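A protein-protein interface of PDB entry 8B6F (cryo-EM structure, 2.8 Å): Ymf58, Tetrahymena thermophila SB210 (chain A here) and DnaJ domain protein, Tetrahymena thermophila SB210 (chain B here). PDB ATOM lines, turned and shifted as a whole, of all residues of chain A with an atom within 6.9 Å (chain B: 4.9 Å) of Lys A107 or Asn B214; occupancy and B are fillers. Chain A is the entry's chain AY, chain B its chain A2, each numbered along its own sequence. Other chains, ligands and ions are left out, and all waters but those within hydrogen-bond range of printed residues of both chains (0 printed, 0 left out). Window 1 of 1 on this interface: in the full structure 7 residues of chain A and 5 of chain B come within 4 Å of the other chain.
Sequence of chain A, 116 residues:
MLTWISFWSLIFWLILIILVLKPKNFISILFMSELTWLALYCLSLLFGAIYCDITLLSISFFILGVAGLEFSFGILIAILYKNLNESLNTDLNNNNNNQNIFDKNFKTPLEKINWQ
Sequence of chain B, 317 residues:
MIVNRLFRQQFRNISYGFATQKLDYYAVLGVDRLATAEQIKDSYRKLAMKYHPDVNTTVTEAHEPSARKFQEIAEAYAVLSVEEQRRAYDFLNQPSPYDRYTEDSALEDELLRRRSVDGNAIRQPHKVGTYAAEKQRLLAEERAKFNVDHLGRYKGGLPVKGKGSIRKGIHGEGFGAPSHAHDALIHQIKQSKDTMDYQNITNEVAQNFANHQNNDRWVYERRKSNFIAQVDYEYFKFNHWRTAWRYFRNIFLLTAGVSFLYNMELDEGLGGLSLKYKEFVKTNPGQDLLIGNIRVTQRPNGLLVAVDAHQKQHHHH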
ATOM      1  N   ASN A  95     -26.123  21.547   6.470  1.00  0.00           N
ATOM      2  CA  ASN A  95     -24.719  21.381   6.818  1.00  0.00           C
ATOM      3  C   ASN A  95     -24.189  22.498   7.708  1.00  0.00           C
ATOM      4  O   ASN A  95     -23.024  22.444   8.112  1.00  0.00           O
ATOM      5  CB  ASN A  95     -23.874  21.297   5.544  1.00  0.00           C
ATOM      6  CG  ASN A  95     -22.465  20.819   5.811  1.00  0.00           C
ATOM      7  OD1 ASN A  95     -22.191  20.206   6.840  1.00  0.00           O
ATOM      8  ND2 ASN A  95     -21.559  21.096   4.880  1.00  0.00           N
ATOM      9  N   ASP A 103     -22.656  15.965  17.987  1.00  0.00           N
ATOM     10  CA  ASP A 103     -22.112  15.049  16.988  1.00  0.00           C
ATOM     11  C   ASP A 103     -22.670  15.346  15.602  1.00  0.00           C
ATOM     12  O   ASP A 103     -23.093  14.448  14.873  1.00  0.00           O
ATOM     13  CB  ASP A 103     -22.407  13.603  17.372  1.00  0.00           C
ATOM     14  CG  ASP A 103     -23.891  13.304  17.416  1.00  0.00           C
ATOM     15  OD1 ASP A 103     -24.680  14.240  17.658  1.00  0.00           O
ATOM     16  OD2 ASP A 103     -24.268  12.132  17.209  1.00  0.00           O
ATOM     17  N   ASN A 105     -21.734  16.196  11.986  1.00  0.00           N
ATOM     18  CA  ASN A 105     -20.545  16.095  11.143  1.00  0.00           C
ATOM     19  C   ASN A 105     -20.950  15.449   9.829  1.00  0.00           C
ATOM     20  O   ASN A 105     -21.397  14.298   9.821  1.00  0.00           O
ATOM     21  CB  ASN A 105     -19.458  15.274  11.844  1.00  0.00           C
ATOM     22  CG  ASN A 105     -18.168  15.203  11.048  1.00  0.00           C
ATOM     23  OD1 ASN A 105     -18.179  15.169   9.818  1.00  0.00           O
ATOM     24  ND2 ASN A 105     -17.043  15.171  11.752  1.00  0.00           N
ATOM     25  N   PHE A 106     -20.790  16.181   8.726  1.00  0.00           N
ATOM     26  CA  PHE A 106     -21.116  15.686   7.396  1.00  0.00           C
ATOM     27  C   PHE A 106     -19.911  15.833   6.482  1.00  0.00           C
ATOM     28  O   PHE A 106     -19.190  16.833   6.543  1.00  0.00           O
ATOM     29  CB  PHE A 106     -22.313  16.436   6.794  1.00  0.00           C
ATOM     30  CG  PHE A 106     -23.616  16.169   7.491  1.00  0.00           C
ATOM     31  CD1 PHE A 106     -23.928  14.903   7.960  1.00  0.00           C
ATOM     32  CD2 PHE A 106     -24.535  17.187   7.672  1.00  0.00           C
ATOM     33  CE1 PHE A 106     -25.128  14.661   8.597  1.00  0.00           C
ATOM     34  CE2 PHE A 106     -25.736  16.951   8.308  1.00  0.00           C
ATOM     35  CZ  PHE A 106     -26.032  15.687   8.772  1.00  0.00           C
ATOM     36  N   LYS A 107     -19.703  14.830   5.633  1.00  0.00           N
ATOM     37  CA  LYS A 107     -18.641  14.832   4.641  1.00  0.00           C
ATOM     38  C   LYS A 107     -19.246  14.585   3.270  1.00  0.00           C
ATOM     39  O   LYS A 107     -20.332  14.016   3.141  1.00  0.00           O
ATOM     40  CB  LYS A 107     -17.583  13.756   4.931  1.00  0.00           C
ATOM     41  CG  LYS A 107     -16.813  13.951   6.221  1.00  0.00           C
ATOM     42  CD  LYS A 107     -15.911  12.759   6.503  1.00  0.00           C
ATOM     43  CE  LYS A 107     -15.016  13.003   7.708  1.00  0.00           C
ATOM     44  NZ  LYS A 107     -15.779  13.453   8.905  1.00  0.00           N
ATOM     45  N   THR A 108     -18.534  15.022   2.241  1.00  0.00           N
ATOM     46  CA  THR A 108     -18.946  14.698   0.887  1.00  0.00           C
ATOM     47  C   THR A 108     -18.864  13.187   0.686  1.00  0.00           C
ATOM     48  O   THR A 108     -17.952  12.541   1.215  1.00  0.00           O
ATOM     49  CB  THR A 108     -18.061  15.409  -0.136  1.00  0.00           C
ATOM     50  OG1 THR A 108     -18.481  15.064  -1.461  1.00  0.00           O
ATOM     51  CG2 THR A 108     -16.606  15.006   0.045  1.00  0.00           C
ATOM     52  N   PRO A 109     -19.786  12.587  -0.061  1.00  0.00           N
ATOM     53  CA  PRO A 109     -19.734  11.133  -0.241  1.00  0.00           C
ATOM     54  C   PRO A 109     -18.600  10.707  -1.160  1.00  0.00           C
ATOM     55  O   PRO A 109     -18.834  10.242  -2.280  1.00  0.00           O
ATOM     56  CB  PRO A 109     -21.109  10.804  -0.834  1.00  0.00           C
ATOM     57  CG  PRO A 109     -21.502  12.033  -1.547  1.00  0.00           C
ATOM     58  CD  PRO A 109     -20.934  13.184  -0.764  1.00  0.00           C
ATOM     59  N   LEU A 110     -17.366  10.868  -0.693  1.00  0.00           N
ATOM     60  CA  LEU A 110     -16.175  10.481  -1.434  1.00  0.00           C
ATOM     61  C   LEU A 110     -15.239   9.712  -0.517  1.00  0.00           C
ATOM     62  O   LEU A 110     -15.401   9.700   0.705  1.00  0.00           O
ATOM     63  CB  LEU A 110     -15.451  11.700  -2.020  1.00  0.00           C
ATOM     64  CG  LEU A 110     -16.154  12.436  -3.161  1.00  0.00           C
ATOM     65  CD1 LEU A 110     -15.335  13.638  -3.585  1.00  0.00           C
ATOM     66  CD2 LEU A 110     -16.392  11.514  -4.345  1.00  0.00           C
ATOM     67  N   ALA B 210     -18.721   3.830   4.442  1.00  0.00           N
ATOM     68  CA  ALA B 210     -18.118   5.041   4.989  1.00  0.00           C
ATOM     69  C   ALA B 210     -19.177   6.055   5.396  1.00  0.00           C
ATOM     70  O   ALA B 210     -19.079   6.673   6.460  1.00  0.00           O
ATOM     71  CB  ALA B 210     -17.157   5.652   3.971  1.00  0.00           C
ATOM     72  N   ASN B 211     -20.203   6.238   4.563  1.00  0.00           N
ATOM     73  CA  ASN B 211     -21.269   7.171   4.910  1.00  0.00           C
ATOM     74  C   ASN B 211     -21.998   6.726   6.170  1.00  0.00           C
ATOM     75  O   ASN B 211     -22.330   7.553   7.027  1.00  0.00           O
ATOM     76  CB  ASN B 211     -22.253   7.313   3.748  1.00  0.00           C
ATOM     77  CG  ASN B 211     -21.590   7.809   2.478  1.00  0.00           C
ATOM     78  OD1 ASN B 211     -21.858   7.304   1.389  1.00  0.00           O
ATOM     79  ND2 ASN B 211     -20.716   8.802   2.612  1.00  0.00           N
ATOM     80  N   HIS B 212     -22.259   5.426   6.301  1.00  0.00           N
ATOM     81  CA  HIS B 212     -22.919   4.929   7.502  1.00  0.00           C
ATOM     82  C   HIS B 212     -22.070   5.177   8.742  1.00  0.00           C
ATOM     83  O   HIS B 212     -22.589   5.581   9.789  1.00  0.00           O
ATOM     84  CB  HIS B 212     -23.222   3.438   7.357  1.00  0.00           C
ATOM     85  CG  HIS B 212     -23.941   2.855   8.533  1.00  0.00           C
ATOM     86  ND1 HIS B 212     -25.271   3.109   8.794  1.00  0.00           N
ATOM     87  CD2 HIS B 212     -23.514   2.037   9.524  1.00  0.00           C
ATOM     88  CE1 HIS B 212     -25.632   2.471   9.891  1.00  0.00           C
ATOM     89  NE2 HIS B 212     -24.585   1.813  10.354  1.00  0.00           N
ATOM     90  N   GLN B 213     -20.761   4.939   8.647  1.00  0.00           N
ATOM     91  CA  GLN B 213     -19.894   5.131   9.805  1.00  0.00           C
ATOM     92  C   GLN B 213     -19.739   6.605  10.158  1.00  0.00           C
ATOM     93  O   GLN B 213     -19.561   6.941  11.333  1.00  0.00           O
ATOM     94  CB  GLN B 213     -18.527   4.503   9.543  1.00  0.00           C
ATOM     95  CG  GLN B 213     -18.571   2.999   9.337  1.00  0.00           C
ATOM     96  CD  GLN B 213     -19.107   2.257  10.543  1.00  0.00           C
ATOM     97  OE1 GLN B 213     -18.727   2.538  11.678  1.00  0.00           O
ATOM     98  NE2 GLN B 213     -20.004   1.308  10.303  1.00  0.00           N
ATOM     99  N   ASN B 214     -19.798   7.496   9.165  1.00  0.00           N
ATOM    100  CA  ASN B 214     -19.637   8.919   9.444  1.00  0.00           C
ATOM    101  C   ASN B 214     -20.719   9.436  10.382  1.00  0.00           C
ATOM    102  O   ASN B 214     -20.505  10.431  11.084  1.00  0.00           O
ATOM    103  CB  ASN B 214     -19.642   9.715   8.140  1.00  0.00           C
ATOM    104  CG  ASN B 214     -18.411   9.457   7.295  1.00  0.00           C
ATOM    105  OD1 ASN B 214     -17.606   8.580   7.604  1.00  0.00           O
ATOM    106  ND2 ASN B 214     -18.258  10.223   6.221  1.00  0.00           N
ATOM    107  N   ASN B 215     -21.885   8.787  10.405  1.00  0.00           N
ATOM    108  CA  ASN B 215     -22.927   9.177  11.351  1.00  0.00           C
ATOM    109  C   ASN B 215     -22.479   8.943  12.788  1.00  0.00           C
ATOM    110  O   ASN B 215     -22.747   9.764  13.672  1.00  0.00           O
ATOM    111  CB  ASN B 215     -24.217   8.408  11.066  1.00  0.00           C
ATOM    112  CG  ASN B 215     -24.857   8.811   9.756  1.00  0.00           C
ATOM    113  OD1 ASN B 215     -24.571   8.236   8.709  1.00  0.00           O
ATOM    114  ND2 ASN B 215     -25.735   9.806   9.811  1.00  0.00           N
ATOM    115  N   ASP B 216     -21.800   7.828  13.040  1.00  0.00           N
ATOM    116  CA  ASP B 216     -21.311   7.479  14.365  1.00  0.00           C
ATOM    117  C   ASP B 216     -19.870   7.916  14.592  1.00  0.00           C
ATOM    118  O   ASP B 216     -19.268   7.518  15.593  1.00  0.00           O
ATOM    119  CB  ASP B 216     -21.430   5.970  14.583  1.00  0.00           C
ATOM    120  CG  ASP B 216     -22.858   5.478  14.482  1.00  0.00           C
ATOM    121  OD1 ASP B 216     -23.756   6.134  15.049  1.00  0.00           O
ATOM    122  OD2 ASP B 216     -23.084   4.440  13.824  1.00  0.00           O
ATOM    123  N   ARG B 217     -19.309   8.721  13.688  1.00  0.00           N
ATOM    124  CA  ARG B 217     -17.924   9.159  13.827  1.00  0.00           C
ATOM    125  C   ARG B 217     -17.648   9.739  15.208  1.00  0.00           C
ATOM    126  O   ARG B 217     -16.585   9.494  15.789  1.00  0.00           O
ATOM    127  CB  ARG B 217     -17.597  10.189  12.746  1.00  0.00           C
ATOM    128  CG  ARG B 217     -16.319  10.974  12.997  1.00  0.00           C
ATOM    129  CD  ARG B 217     -15.966  11.840  11.802  1.00  0.00           C
ATOM    130  NE  ARG B 217     -15.625  11.040  10.632  1.00  0.00           N
ATOM    131  CZ  ARG B 217     -14.421  10.546  10.381  1.00  0.00           C
ATOM    132  NH1 ARG B 217     -13.406  10.742  11.208  1.00  0.00           N
ATOM    133  NH2 ARG B 217     -14.228   9.837   9.274  1.00  0.00           N
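NZ of Lys A107 sits close to NE of Arg B217 (3.0 Å).
Of chain B, only Asn B214 and Arg B217 come within 4 Å of Lys A107.
Asn B214 touches just one residue of chain A: Lys A107.
Printed residues of chain B within 4 Å of Pro A109: Asn B211.
Of the printed residues of chain A, Asn B211 touches Pro A109 (3.8 Å).
Of the printed residues of chain A, Arg B217 touches Asn A105 (3.5 Å) and Lys A107 (3.0 Å).
Of the printed residues of chain B, Asn A105 touches Arg B217.
The nearest printed residue of chain B that does not touch Lys A107 is Asn B211 (5.3 Å).
Of the 8 printed residues of chain B, 3 touch a printed residue of chain A.
Printed residues of chain B that touch a printed residue of chain A: Asn B211, Asn B214 and Arg B217.
Among the printed residues, 4 pairs touch across the chains.
O of Asn B211 sits close to OD1 of Asn B215.
The backbone carbonyl oxygen (O) of Ala B210 lies close to the side-chain amide oxygen (OD1) of Asn B214 (2.7 Å).
NZ of Lys A107 sits at hydrogen-bond distance from OD1 of Asn A105 (3.1 Å).
Among the printed residues, merely in contact across the chains: Lys A107 with Asn B214 (3.5 Å), Asn A105 with Arg B217 (3.5 Å) and Pro A109 with Asn B211 (3.8 Å).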
